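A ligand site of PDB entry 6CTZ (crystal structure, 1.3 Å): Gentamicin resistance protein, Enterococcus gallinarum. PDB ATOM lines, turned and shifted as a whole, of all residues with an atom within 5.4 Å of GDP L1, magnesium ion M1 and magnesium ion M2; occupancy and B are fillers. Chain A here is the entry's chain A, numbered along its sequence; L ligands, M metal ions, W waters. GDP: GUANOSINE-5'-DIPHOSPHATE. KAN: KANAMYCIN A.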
ATOM      1  N   LEU A  23      -0.924   5.265 -35.069  1.00  0.00           N
ATOM      2  CA  LEU A  23      -1.980   4.941 -34.128  1.00  0.00           C
ATOM      3  C   LEU A  23      -2.853   6.143 -33.794  1.00  0.00           C
ATOM      4  O   LEU A  23      -4.089   6.045 -33.815  1.00  0.00           O
ATOM      5  CB  LEU A  23      -1.372   4.357 -32.845  1.00  0.00           C
ATOM      6  CG  LEU A  23      -2.366   3.955 -31.749  1.00  0.00           C
ATOM      7  CD1 LEU A  23      -3.304   2.864 -32.249  1.00  0.00           C
ATOM      8  CD2 LEU A  23      -1.610   3.499 -30.514  1.00  0.00           C
ATOM      9  N   GLY A  24      -2.252   7.284 -33.495  1.00  0.00           N
ATOM     10  CA  GLY A  24      -3.024   8.472 -33.210  1.00  0.00           C
ATOM     11  C   GLY A  24      -2.097   9.636 -32.963  1.00  0.00           C
ATOM     12  O   GLY A  24      -0.878   9.486 -32.857  1.00  0.00           O
ATOM     13  N   GLU A  25      -2.695  10.819 -32.861  1.00  0.00           N
ATOM     14  CA  GLU A  25      -1.925  12.016 -32.588  1.00  0.00           C
ATOM     15  C   GLU A  25      -2.834  13.071 -31.984  1.00  0.00           C
ATOM     16  O   GLU A  25      -4.037  13.113 -32.269  1.00  0.00           O
ATOM     17  CB  GLU A  25      -1.220  12.551 -33.841  1.00  0.00           C
ATOM     18  CG  GLU A  25      -2.114  13.306 -34.791  1.00  0.00           C
ATOM     19  CD  GLU A  25      -1.362  13.858 -35.980  1.00  0.00           C
ATOM     20  OE1 GLU A  25      -1.682  13.477 -37.119  1.00  0.00           O
ATOM     21  OE2 GLU A  25      -0.428  14.667 -35.769  1.00  0.00           O
ATOM     22  N   GLY A  26      -2.243  13.886 -31.120  1.00  0.00           N
ATOM     23  CA  GLY A  26      -2.943  15.035 -30.575  1.00  0.00           C
ATOM     24  C   GLY A  26      -2.090  16.276 -30.710  1.00  0.00           C
ATOM     25  O   GLY A  26      -1.189  16.328 -31.552  1.00  0.00           O
ATOM     26  N   PHE A  27      -2.343  17.295 -29.921  1.00  0.00           N
ATOM     27  CA  PHE A  27      -1.613  18.524 -30.018  1.00  0.00           C
ATOM     28  C   PHE A  27      -0.173  18.396 -29.563  1.00  0.00           C
ATOM     29  O   PHE A  27       0.613  19.159 -29.962  1.00  0.00           O
ATOM     30  CB  PHE A  27      -2.246  19.642 -29.136  1.00  0.00           C
ATOM     31  CG  PHE A  27      -3.602  20.176 -29.578  1.00  0.00           C
ATOM     32  CD1 PHE A  27      -4.317  19.635 -30.588  1.00  0.00           C
ATOM     33  CD2 PHE A  27      -4.150  21.259 -28.934  1.00  0.00           C
ATOM     34  CE1 PHE A  27      -5.563  20.145 -30.950  1.00  0.00           C
ATOM     35  CE2 PHE A  27      -5.384  21.756 -29.271  1.00  0.00           C
ATOM     36  CZ  PHE A  27      -6.074  21.210 -30.308  1.00  0.00           C
ATOM     37  N   ARG A  28       0.138  17.419 -28.730  1.00  0.00           N
ATOM     38  CA  ARG A  28       1.457  17.309 -28.148  1.00  0.00           C
ATOM     39  C   ARG A  28       2.275  16.060 -28.434  1.00  0.00           C
ATOM     40  O   ARG A  28       3.415  16.040 -28.156  1.00  0.00           O
ATOM     41  CB  ARG A  28       1.305  17.492 -26.612  1.00  0.00           C
ATOM     42  CG  ARG A  28       0.762  18.853 -26.191  1.00  0.00           C
ATOM     43  CD  ARG A  28       1.860  19.803 -25.782  1.00  0.00           C
ATOM     44  NE  ARG A  28       1.591  21.235 -26.005  1.00  0.00           N
ATOM     45  CZ  ARG A  28       1.160  22.096 -25.119  1.00  0.00           C
ATOM     46  NH1 ARG A  28       0.866  21.730 -23.892  1.00  0.00           N
ATOM     47  NH2 ARG A  28       1.002  23.336 -25.440  1.00  0.00           N
ATOM     48  N   ASN A  29       1.655  15.039 -28.964  1.00  0.00           N
ATOM     49  CA  ASN A  29       2.323  13.771 -29.203  1.00  0.00           C
ATOM     50  C   ASN A  29       1.862  13.049 -30.440  1.00  0.00           C
ATOM     51  O   ASN A  29       0.748  13.117 -30.813  1.00  0.00           O
ATOM     52  CB  ASN A  29       2.074  12.803 -28.031  1.00  0.00           C
ATOM     53  CG  ASN A  29       2.669  13.276 -26.747  1.00  0.00           C
ATOM     54  OD1 ASN A  29       3.830  13.171 -26.532  1.00  0.00           O
ATOM     55  ND2 ASN A  29       1.864  13.849 -25.932  1.00  0.00           N
ATOM     56  N   TYR A  30       2.785  12.330 -31.053  1.00  0.00           N
ATOM     57  CA  TYR A  30       2.505  11.428 -32.166  1.00  0.00           C
ATOM     58  C   TYR A  30       2.742  10.009 -31.691  1.00  0.00           C
ATOM     59  O   TYR A  30       3.810   9.702 -31.152  1.00  0.00           O
ATOM     60  CB  TYR A  30       3.436  11.773 -33.334  1.00  0.00           C
ATOM     61  CG  TYR A  30       3.343  10.851 -34.525  1.00  0.00           C
ATOM     62  CD1 TYR A  30       2.145  10.672 -35.203  1.00  0.00           C
ATOM     63  CD2 TYR A  30       4.464  10.175 -34.980  1.00  0.00           C
ATOM     64  CE1 TYR A  30       2.065   9.832 -36.300  1.00  0.00           C
ATOM     65  CE2 TYR A  30       4.397   9.344 -36.092  1.00  0.00           C
ATOM     66  CZ  TYR A  30       3.196   9.164 -36.739  1.00  0.00           C
ATOM     67  OH  TYR A  30       3.124   8.335 -37.835  1.00  0.00           O
ATOM     68  N   ALA A  31       1.745   9.142 -31.856  1.00  0.00           N
ATOM     69  CA  ALA A  31       1.807   7.770 -31.364  1.00  0.00           C
ATOM     70  C   ALA A  31       1.775   6.799 -32.533  1.00  0.00           C
ATOM     71  O   ALA A  31       0.948   6.939 -33.442  1.00  0.00           O
ATOM     72  CB  ALA A  31       0.668   7.460 -30.399  1.00  0.00           C
ATOM     73  N   VAL A  39       3.073   0.828 -28.057  1.00  0.00           N
ATOM     74  CA  VAL A  39       2.839   2.181 -28.462  1.00  0.00           C
ATOM     75  C   VAL A  39       4.122   2.982 -28.210  1.00  0.00           C
ATOM     76  O   VAL A  39       4.607   3.008 -27.124  1.00  0.00           O
ATOM     77  CB  VAL A  39       1.680   2.837 -27.630  1.00  0.00           C
ATOM     78  CG1 VAL A  39       1.529   4.309 -27.993  1.00  0.00           C
ATOM     79  CG2 VAL A  39       0.382   2.078 -27.787  1.00  0.00           C
ATOM     80  N   ARG A  41       5.488   6.823 -28.341  1.00  0.00           N
ATOM     81  CA  ARG A  41       4.812   8.104 -28.261  1.00  0.00           C
ATOM     82  C   ARG A  41       5.868   9.197 -28.237  1.00  0.00           C
ATOM     83  O   ARG A  41       6.707   9.234 -27.321  1.00  0.00           O
ATOM     84  CB  ARG A  41       3.911   8.135 -27.028  1.00  0.00           C
ATOM     85  CG  ARG A  41       3.020   9.350 -26.924  1.00  0.00           C
ATOM     86  CD  ARG A  41       2.162   9.155 -25.698  1.00  0.00           C
ATOM     87  NE  ARG A  41       1.308  10.237 -25.251  1.00  0.00           N
ATOM     88  CZ  ARG A  41       1.531  10.953 -24.149  1.00  0.00           C
ATOM     89  NH1 ARG A  41       2.660  10.791 -23.463  1.00  0.00           N
ATOM     90  NH2 ARG A  41       0.638  11.828 -23.728  1.00  0.00           N
ATOM     91  N   LYS A  44       5.734  16.400 -29.733  1.00  0.00           N
ATOM     92  CA  LYS A  44       5.758  17.261 -30.906  1.00  0.00           C
ATOM     93  C   LYS A  44       6.384  18.619 -30.642  1.00  0.00           C
ATOM     94  O   LYS A  44       6.489  19.429 -31.583  1.00  0.00           O
ATOM     95  CB  LYS A  44       4.330  17.421 -31.465  1.00  0.00           C
ATOM     96  CG  LYS A  44       3.758  16.133 -32.051  1.00  0.00           C
ATOM     97  CD  LYS A  44       2.243  16.201 -32.267  1.00  0.00           C
ATOM     98  CE  LYS A  44       1.851  17.319 -33.220  1.00  0.00           C
ATOM     99  NZ  LYS A  44       0.408  17.241 -33.596  1.00  0.00           N
ATOM    100  N   GLU A  51       5.703  17.853 -20.669  1.00  0.00           N
ATOM    101  CA  GLU A  51       4.561  17.069 -20.199  1.00  0.00           C
ATOM    102  C   GLU A  51       4.919  15.590 -20.105  1.00  0.00           C
ATOM    103  O   GLU A  51       4.489  14.899 -19.172  1.00  0.00           O
ATOM    104  CB  GLU A  51       3.349  17.307 -21.103  1.00  0.00           C
ATOM    105  CG  GLU A  51       2.863  18.758 -21.029  1.00  0.00           C
ATOM    106  CD  GLU A  51       1.718  19.112 -21.973  1.00  0.00           C
ATOM    107  OE1 GLU A  51       1.321  18.274 -22.814  1.00  0.00           O
ATOM    108  OE2 GLU A  51       1.206  20.230 -21.857  1.00  0.00           O
ATOM    109  N   TYR A  88       5.199   1.973 -24.472  1.00  0.00           N
ATOM    110  CA  TYR A  88       4.401   1.251 -23.520  1.00  0.00           C
ATOM    111  C   TYR A  88       3.515   0.227 -24.195  1.00  0.00           C
ATOM    112  O   TYR A  88       3.165   0.424 -25.302  1.00  0.00           O
ATOM    113  CB  TYR A  88       3.539   2.216 -22.667  1.00  0.00           C
ATOM    114  CG  TYR A  88       2.621   3.212 -23.393  1.00  0.00           C
ATOM    115  CD1 TYR A  88       3.079   4.441 -23.737  1.00  0.00           C
ATOM    116  CD2 TYR A  88       1.289   2.932 -23.625  1.00  0.00           C
ATOM    117  CE1 TYR A  88       2.263   5.365 -24.314  1.00  0.00           C
ATOM    118  CE2 TYR A  88       0.466   3.873 -24.219  1.00  0.00           C
ATOM    119  CZ  TYR A  88       0.968   5.090 -24.521  1.00  0.00           C
ATOM    120  OH  TYR A  88       0.199   6.075 -25.081  1.00  0.00           O
ATOM    121  N   ARG A  89       3.190  -0.851 -23.506  1.00  0.00           N
ATOM    122  CA  ARG A  89       2.298  -1.853 -24.056  1.00  0.00           C
ATOM    123  C   ARG A  89       0.973  -1.133 -24.299  1.00  0.00           C
ATOM    124  O   ARG A  89       0.489  -0.440 -23.449  1.00  0.00           O
ATOM    125  CB  ARG A  89       2.073  -3.033 -23.122  1.00  0.00           C
ATOM    126  CG  ARG A  89       3.236  -4.022 -23.067  1.00  0.00           C
ATOM    127  CD  ARG A  89       2.865  -5.450 -22.656  1.00  0.00           C
ATOM    128  NE  ARG A  89       3.982  -6.385 -22.964  1.00  0.00           N
ATOM    129  CZ  ARG A  89       4.138  -7.037 -24.122  1.00  0.00           C
ATOM    130  NH1 ARG A  89       3.284  -6.901 -25.101  1.00  0.00           N
ATOM    131  NH2 ARG A  89       5.176  -7.832 -24.314  1.00  0.00           N
ATOM    132  N   LYS A  90       0.382  -1.354 -25.450  1.00  0.00           N
ATOM    133  CA  LYS A  90      -0.875  -0.705 -25.795  1.00  0.00           C
ATOM    134  C   LYS A  90      -1.898  -0.903 -24.677  1.00  0.00           C
ATOM    135  O   LYS A  90      -2.077  -2.004 -24.143  1.00  0.00           O
ATOM    136  CB  LYS A  90      -1.386  -1.300 -27.101  1.00  0.00           C
ATOM    137  CG  LYS A  90      -2.553  -0.547 -27.692  1.00  0.00           C
ATOM    138  CD  LYS A  90      -2.971  -1.117 -29.036  1.00  0.00           C
ATOM    139  CE  LYS A  90      -3.601  -2.481 -28.886  1.00  0.00           C
ATOM    140  NZ  LYS A  90      -4.249  -2.908 -30.157  1.00  0.00           N
ATOM    141  N   VAL A  91      -2.533   0.193 -24.282  1.00  0.00           N
ATOM    142  CA  VAL A  91      -3.633   0.078 -23.338  1.00  0.00           C
ATOM    143  C   VAL A  91      -4.804  -0.504 -24.119  1.00  0.00           C
ATOM    144  O   VAL A  91      -5.227   0.052 -25.134  1.00  0.00           O
ATOM    145  CB  VAL A  91      -3.945   1.448 -22.698  1.00  0.00           C
ATOM    146  CG1 VAL A  91      -5.102   1.344 -21.720  1.00  0.00           C
ATOM    147  CG2 VAL A  91      -2.698   1.994 -21.991  1.00  0.00           C
ATOM    148  N   GLY A  93      -8.281  -2.178 -25.603  1.00  0.00           N
ATOM    149  CA  GLY A  93      -9.669  -1.807 -25.692  1.00  0.00           C
ATOM    150  C   GLY A  93      -9.949  -0.945 -26.907  1.00  0.00           C
ATOM    151  O   GLY A  93      -9.067  -0.645 -27.717  1.00  0.00           O
ATOM    152  N   ILE A  95     -11.089   2.687 -28.129  1.00  0.00           N
ATOM    153  CA  ILE A  95     -11.300   4.074 -27.751  1.00  0.00           C
ATOM    154  C   ILE A  95     -12.766   4.421 -27.945  1.00  0.00           C
ATOM    155  O   ILE A  95     -13.332   4.160 -29.014  1.00  0.00           O
ATOM    156  CB  ILE A  95     -10.405   5.008 -28.588  1.00  0.00           C
ATOM    157  CG1 ILE A  95      -8.927   4.727 -28.305  1.00  0.00           C
ATOM    158  CG2 ILE A  95     -10.762   6.471 -28.346  1.00  0.00           C
ATOM    159  CD1 ILE A  95      -7.995   5.601 -29.097  1.00  0.00           C
ATOM    160  N   ASP A 192      -7.354  16.546 -19.086  1.00  0.00           N
ATOM    161  CA  ASP A 192      -7.785  16.456 -20.479  1.00  0.00           C
ATOM    162  C   ASP A 192      -8.697  15.235 -20.603  1.00  0.00           C
ATOM    163  O   ASP A 192      -8.486  14.344 -21.441  1.00  0.00           O
ATOM    164  CB  ASP A 192      -6.565  16.388 -21.401  1.00  0.00           C
ATOM    165  CG  ASP A 192      -6.884  16.754 -22.838  1.00  0.00           C
ATOM    166  OD1 ASP A 192      -7.851  17.502 -23.090  1.00  0.00           O
ATOM    167  OD2 ASP A 192      -6.120  16.302 -23.726  1.00  0.00           O
ATOM    168  N   ASP A 196     -11.994  10.559 -26.135  1.00  0.00           N
ATOM    169  CA  ASP A 196     -10.920  10.067 -26.992  1.00  0.00           C
ATOM    170  C   ASP A 196      -9.769   9.446 -26.194  1.00  0.00           C
ATOM    171  O   ASP A 196      -8.845   8.885 -26.795  1.00  0.00           O
ATOM    172  CB  ASP A 196     -10.411  11.172 -27.938  1.00  0.00           C
ATOM    173  CG  ASP A 196      -9.724  12.299 -27.205  1.00  0.00           C
ATOM    174  OD1 ASP A 196     -10.033  12.520 -26.027  1.00  0.00           O
ATOM    175  OD2 ASP A 196      -8.852  12.974 -27.804  1.00  0.00           O
ATOM    176  N   HIS A 197      -9.834   9.508 -24.866  1.00  0.00           N
ATOM    177  CA  HIS A 197      -8.851   8.926 -23.973  1.00  0.00           C
ATOM    178  C   HIS A 197      -9.427   7.783 -23.145  1.00  0.00           C
ATOM    179  O   HIS A 197      -8.722   7.253 -22.284  1.00  0.00           O
ATOM    180  CB  HIS A 197      -8.292   9.983 -23.025  1.00  0.00           C
ATOM    181  CG  HIS A 197      -7.533  11.066 -23.712  1.00  0.00           C
ATOM    182  ND1 HIS A 197      -7.518  12.363 -23.260  1.00  0.00           N
ATOM    183  CD2 HIS A 197      -6.749  11.040 -24.815  1.00  0.00           C
ATOM    184  CE1 HIS A 197      -6.749  13.091 -24.050  1.00  0.00           C
ATOM    185  NE2 HIS A 197      -6.268  12.317 -25.002  1.00  0.00           N
ATOM    186  N   LEU A 199     -10.549   4.039 -22.862  1.00  0.00           N
ATOM    187  CA  LEU A 199     -10.474   2.718 -23.483  1.00  0.00           C
ATOM    188  C   LEU A 199     -11.510   1.822 -22.844  1.00  0.00           C
ATOM    189  O   LEU A 199     -11.640   1.787 -21.620  1.00  0.00           O
ATOM    190  CB  LEU A 199      -9.075   2.124 -23.315  1.00  0.00           C
ATOM    191  CG  LEU A 199      -7.942   2.599 -24.228  1.00  0.00           C
ATOM    192  CD1 LEU A 199      -8.177   2.169 -25.689  1.00  0.00           C
ATOM    193  CD2 LEU A 199      -7.681   4.105 -24.076  1.00  0.00           C
ATOM    194  N   ILE A 213      -5.847   7.074 -21.027  1.00  0.00           N
ATOM    195  CA  ILE A 213      -4.551   7.485 -21.546  1.00  0.00           C
ATOM    196  C   ILE A 213      -4.355   9.003 -21.463  1.00  0.00           C
ATOM    197  O   ILE A 213      -5.256   9.732 -21.028  1.00  0.00           O
ATOM    198  CB  ILE A 213      -4.335   6.964 -22.982  1.00  0.00           C
ATOM    199  CG1 ILE A 213      -5.431   7.493 -23.916  1.00  0.00           C
ATOM    200  CG2 ILE A 213      -4.265   5.430 -22.992  1.00  0.00           C
ATOM    201  CD1 ILE A 213      -5.117   7.295 -25.385  1.00  0.00           C
ATOM    202  N   ASP A 214      -3.173   9.463 -21.862  1.00  0.00           N
ATOM    203  CA  ASP A 214      -2.816  10.867 -22.041  1.00  0.00           C
ATOM    204  C   ASP A 214      -2.970  11.735 -20.796  1.00  0.00           C
ATOM    205  O   ASP A 214      -3.917  12.520 -20.687  1.00  0.00           O
ATOM    206  CB  ASP A 214      -3.552  11.519 -23.205  1.00  0.00           C
ATOM    207  CG  ASP A 214      -2.963  12.876 -23.572  1.00  0.00           C
ATOM    208  OD1 ASP A 214      -1.907  13.264 -22.995  1.00  0.00           O
ATOM    209  OD2 ASP A 214      -3.561  13.567 -24.443  1.00  0.00           O
ATOM    210  N   GLY A 216      -0.875  14.107 -20.016  1.00  0.00           N
ATOM    211  CA  GLY A 216       0.016  15.225 -20.234  1.00  0.00           C
ATOM    212  C   GLY A 216      -0.452  16.541 -19.644  1.00  0.00           C
ATOM    213  O   GLY A 216       0.373  17.423 -19.381  1.00  0.00           O
ATOM    214  N   ASP A 217      -1.760  16.699 -19.431  1.00  0.00           N
ATOM    215  CA  ASP A 217      -2.310  17.904 -18.820  1.00  0.00           C
ATOM    216  C   ASP A 217      -2.496  17.763 -17.320  1.00  0.00           C
ATOM    217  O   ASP A 217      -3.137  18.617 -16.708  1.00  0.00           O
ATOM    218  CB  ASP A 217      -3.612  18.311 -19.511  1.00  0.00           C
ATOM    219  CG  ASP A 217      -3.372  18.890 -20.888  1.00  0.00           C
ATOM    220  OD1 ASP A 217      -2.625  19.879 -21.007  1.00  0.00           O
ATOM    221  OD2 ASP A 217      -3.940  18.358 -21.859  1.00  0.00           O
HETATM  222  PB  GDP L   1      -1.727  14.039 -27.202  1.00  0.00           P
HETATM  223  O1B GDP L   1      -1.096  14.336 -25.867  1.00  0.00           O
HETATM  224  O2B GDP L   1      -3.226  14.238 -27.193  1.00  0.00           O
HETATM  225  O3B GDP L   1      -1.022  14.751 -28.335  1.00  0.00           O
HETATM  226  O3A GDP L   1      -1.429  12.464 -27.465  1.00  0.00           O
HETATM  227  PA  GDP L   1      -2.139  11.169 -26.797  1.00  0.00           P
HETATM  228  O1A GDP L   1      -1.352  10.689 -25.610  1.00  0.00           O
HETATM  229  O2A GDP L   1      -3.602  11.468 -26.508  1.00  0.00           O
HETATM  230  O5' GDP L   1      -1.945  10.076 -27.982  1.00  0.00           O
HETATM  231  C5' GDP L   1      -2.437  10.381 -29.282  1.00  0.00           C
HETATM  232  C4' GDP L   1      -3.461   9.346 -29.673  1.00  0.00           C
HETATM  233  O4' GDP L   1      -2.803   8.089 -29.818  1.00  0.00           O
HETATM  234  C3' GDP L   1      -4.542   9.089 -28.643  1.00  0.00           C
HETATM  235  O3' GDP L   1      -5.587  10.075 -28.673  1.00  0.00           O
HETATM  236  C2' GDP L   1      -5.036   7.740 -29.095  1.00  0.00           C
HETATM  237  O2' GDP L   1      -5.849   7.865 -30.268  1.00  0.00           O
HETATM  238  C1' GDP L   1      -3.742   7.065 -29.524  1.00  0.00           C
HETATM  239  N9  GDP L   1      -3.197   6.270 -28.406  1.00  0.00           N
HETATM  240  C8  GDP L   1      -2.206   6.611 -27.550  1.00  0.00           C
HETATM  241  N7  GDP L   1      -1.995   5.593 -26.669  1.00  0.00           N
HETATM  242  C5  GDP L   1      -2.866   4.608 -26.966  1.00  0.00           C
HETATM  243  C6  GDP L   1      -3.192   3.280 -26.440  1.00  0.00           C
HETATM  244  O6  GDP L   1      -2.574   2.807 -25.469  1.00  0.00           O
HETATM  245  N1  GDP L   1      -4.174   2.605 -27.067  1.00  0.00           N
HETATM  246  C2  GDP L   1      -4.863   3.091 -28.127  1.00  0.00           C
HETATM  247  N2  GDP L   1      -5.818   2.333 -28.691  1.00  0.00           N
HETATM  248  N3  GDP L   1      -4.619   4.302 -28.657  1.00  0.00           N
HETATM  249  C4  GDP L   1      -3.642   5.064 -28.109  1.00  0.00           C
HETATM  250  C1  KAN L   2     -12.363  20.847 -29.499  1.00  0.00           C
HETATM  251  C2  KAN L   2     -13.484  21.877 -29.513  1.00  0.00           C
HETATM  252  C3  KAN L   2     -14.797  21.194 -29.869  1.00  0.00           C
HETATM  253  C4  KAN L   2     -14.612  20.562 -31.241  1.00  0.00           C
HETATM  254  C5  KAN L   2     -13.455  19.567 -31.231  1.00  0.00           C
HETATM  255  C6  KAN L   2     -13.205  18.978 -32.615  1.00  0.00           C
HETATM  256  C7  KAN L   2     -10.203  17.646 -25.871  1.00  0.00           C
HETATM  257  C8  KAN L   2      -9.452  18.570 -26.814  1.00  0.00           C
HETATM  258  C9  KAN L   2     -10.405  19.623 -27.387  1.00  0.00           C
HETATM  259  C10 KAN L   2     -11.597  18.974 -28.094  1.00  0.00           C
HETATM  260  C11 KAN L   2     -12.300  17.997 -27.158  1.00  0.00           C
HETATM  261  C12 KAN L   2     -11.342  16.946 -26.614  1.00  0.00           C
HETATM  262  C13 KAN L   2      -7.294  19.697 -26.736  1.00  0.00           C
HETATM  263  C14 KAN L   2      -6.015  19.512 -25.931  1.00  0.00           C
HETATM  264  C15 KAN L   2      -6.166  20.248 -24.596  1.00  0.00           C
HETATM  265  C16 KAN L   2      -6.492  21.711 -24.861  1.00  0.00           C
HETATM  266  C17 KAN L   2      -7.717  21.816 -25.755  1.00  0.00           C
HETATM  267  C18 KAN L   2      -7.954  23.272 -26.117  1.00  0.00           C
HETATM  268  N1  KAN L   2     -12.068  18.086 -32.538  1.00  0.00           N
HETATM  269  N2  KAN L   2     -13.408  17.325 -27.831  1.00  0.00           N
HETATM  270  N3  KAN L   2      -9.273  16.658 -25.314  1.00  0.00           N
HETATM  271  N4  KAN L   2      -4.967  20.155 -23.769  1.00  0.00           N
HETATM  272  O5  KAN L   2     -12.239  20.133 -30.735  1.00  0.00           O
HETATM  273  O6  KAN L   2     -13.586  22.467 -28.217  1.00  0.00           O
HETATM  274  O7  KAN L   2     -15.869  22.149 -29.918  1.00  0.00           O
HETATM  275  O8  KAN L   2     -15.822  19.884 -31.605  1.00  0.00           O
HETATM  276  O9  KAN L   2     -12.594  19.950 -28.414  1.00  0.00           O
HETATM  277  O10 KAN L   2      -9.697  20.423 -28.356  1.00  0.00           O
HETATM  278  O11 KAN L   2      -8.411  19.177 -26.022  1.00  0.00           O
HETATM  279  O12 KAN L   2      -7.496  21.094 -26.948  1.00  0.00           O
HETATM  280  O13 KAN L   2      -5.804  18.114 -25.764  1.00  0.00           O
HETATM  281  O14 KAN L   2      -6.776  22.422 -23.646  1.00  0.00           O
HETATM  282  O15 KAN L   2      -9.118  23.367 -26.956  1.00  0.00           O
HETATM  283 MG    MG M   1      -4.654  13.171 -26.199  1.00  0.00          MG
HETATM  284 MG    MG M   2      -1.911  15.115 -24.190  1.00  0.00          MG
HETATM  285  O   HOH W   1      -0.007  15.741 -23.422  1.00  0.00           O
HETATM  286  O   HOH W   2      -2.329  16.877 -25.160  1.00  0.00           O
HETATM  287  O   HOH W   3      -6.250   5.746 -32.010  1.00  0.00           O
HETATM  288  O   HOH W   4      -8.289   8.972 -29.519  1.00  0.00           O
HETATM  289  O   HOH W   5      -6.381  -0.331 -27.735  1.00  0.00           O
HETATM  290  O   HOH W   6      -5.602  15.034 -25.989  1.00  0.00           O
HETATM  291  O   HOH W   7      -1.053   8.481 -23.741  1.00  0.00           O
HETATM  292  O   HOH W   8      -7.230  11.182 -31.034  1.00  0.00           O
HETATM  293  O   HOH W   9      -7.062   3.128 -31.248  1.00  0.00           O
HETATM  294  O   HOH W  10      -5.837  12.825 -27.840  1.00  0.00           O
HETATM  295  O   HOH W  11      -3.889  16.848 -27.517  1.00  0.00           O
HETATM  296  O   HOH W  12      -3.204  15.842 -22.631  1.00  0.00           O
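O1A of GDP L1 lies within salt-bridge range of NE of Arg 41 (2.7 Å).
N7 of GDP L1 is in hydrogen-bond range of OH of Tyr 88, 2.8 Å away.
An oxygen (O3B) of GDP L1 lies within hydrogen-bond range of the backbone NH (N) of Asn 29, 2.8 Å away.
An oxygen (O1B) of GDP L1 sits close to the side-chain amide nitrogen of Asn 29 (3.0 Å).
An oxygen (O6) of GDP L1 lies within hydrogen-bond range of the backbone NH (N) of Val 91 (2.9 Å).
N1 of GDP L1 lies within hydrogen-bond range of O of Val 91 (3.4 Å).
N of Arg 28 lies within hydrogen-bond range of O3B of GDP L1 (2.9 Å).
The backbone NH (N) of Gly 26 sits close to an oxygen (O3B) of GDP L1 (3.2 Å).
N of Phe 27 lies within hydrogen-bond range of O3B of GDP L1, at 3.3 Å.
A nitrogen (N3) of KAN L2 lies within salt-bridge range of the side-chain carboxylate of Asp 192.
The side-chain carboxylate (OD2) of Asp 217 is in salt-bridge range of a nitrogen (N4) of KAN L2 (2.8 Å).
Magnesium ion M1 is bound by O2A of GDP L1 (2.0 Å), O2B of GDP L1 (2.0 Å), water W10 (2.1 Å), water W6 (2.1 Å), OD2 of Asp 214 (2.1 Å) and NE2 of His 197 (2.2 Å).
Two residues have an atom within 4 Å of magnesium ion M1: His 197 and Asp 214.
The side-chain carboxylate of Asp 214 sits close to the backbone NH of Gly 216, at 3.3 Å.
O of His 197 is in hydrogen-bond range of N of Ile 213, at 3.1 Å.
A ring nitrogen (ND1) of His 197 lies within hydrogen-bond range of the backbone carbonyl oxygen (O) of Asp 192, 2.9 Å away.
NH2 of Arg 41 lies close to ND2 of Asn 29 (3.2 Å).
The backbone NH (N) of Val 39 is in hydrogen-bond range of the backbone carbonyl oxygen (O) of Tyr 88 (2.8 Å).
The side-chain carboxylate (OE2) of Glu 51 lies within salt-bridge range of the guanidinium group (NH1) of Arg 28, at 2.6 Å.
The backbone NH (N) of Leu 23 is in hydrogen-bond range of the backbone carbonyl oxygen (O) of Ala 31 (3.0 Å).
OE2 of Glu 25 is in salt-bridge range of NZ of Lys 44 (3.5 Å).
Magnesium ion M2 is bound by an oxygen (O1B) of GDP L1 (2.0 Å), water W2 (2.1 Å), water W1 (2.1 Å), water W12 (2.2 Å), the side-chain carboxylate (OD1) of Asp 214 (2.2 Å) and the side-chain carboxylate (OD2) of Asp 214 (2.3 Å).
Magnesium ion M2 has six donor atoms within binding distance.
Leu 23 touches GDP L1 (CD2 to C4, 3.5 Å).
Gly 24 touches GDP L1 (CA to O4', 3.4 Å).
Glu 25 touches GDP L1 (N to C4', 3.6 Å).
Ala 31 touches GDP L1 (CB to O4', 3.6 Å).
CG2 of Val 39 touches O6 of GDP L1, at 3.8 Å.
Lys 90 touches GDP L1 (CG to N1, 3.6 Å).
CD1 of Ile 95 touches O2' of GDP L1, at 3.3 Å.
Asp 196 touches GDP L1 (O to O3', 3.9 Å).
Leu 199 touches GDP L1.
Ile 213 touches GDP L1.
Hydrophobic or aromatic side chains that line GDP L1: Leu 23, Ala 31, Val 39, Tyr 88, Val 91, Ile 95, His 197, Leu 199 and Ile 213.
19 residues have an atom within 4 Å of GDP L1: Leu 23, Gly 24, Glu 25, Gly 26, Phe 27, Arg 28, Asn 29, Ala 31, Val 39, Arg 41, Tyr 88, Lys 90, Val 91, Ile 95, Asp 196, His 197, Leu 199, Ile 213 and Asp 214.
One residue has an atom within 4 Å of magnesium ion M2: Asp 214.
The nearest printed residue that does not touch magnesium ion M2 is Arg 41 (4.2 Å).
Water W10 bridges O3' of GDP L1 and OD2 of Asp 196.
Water W6 lies within hydrogen-bond range of OD2 of Asp 192 and O13 of KAN L2.
Water W12 bridges OD2 of Asp 217 (2.7 Å) and OD2 of Asp 192 (3.1 Å).
Water W11 lies within hydrogen-bond range of an oxygen (O13) of KAN L2 (2.9 Å) and the backbone NH (N) of Phe 27 (2.9 Å).
Water W3 lies within hydrogen-bond range of O2' of GDP L1 and O of Leu 23.
Water W7 lies within hydrogen-bond range of an oxygen (O1A) of GDP L1 (2.9 Å), the backbone NH of Asp 214 (3.0 Å), the side-chain hydroxyl of Tyr 88 (3.0 Å) and the guanidinium group of Arg 41 (3.3 Å).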
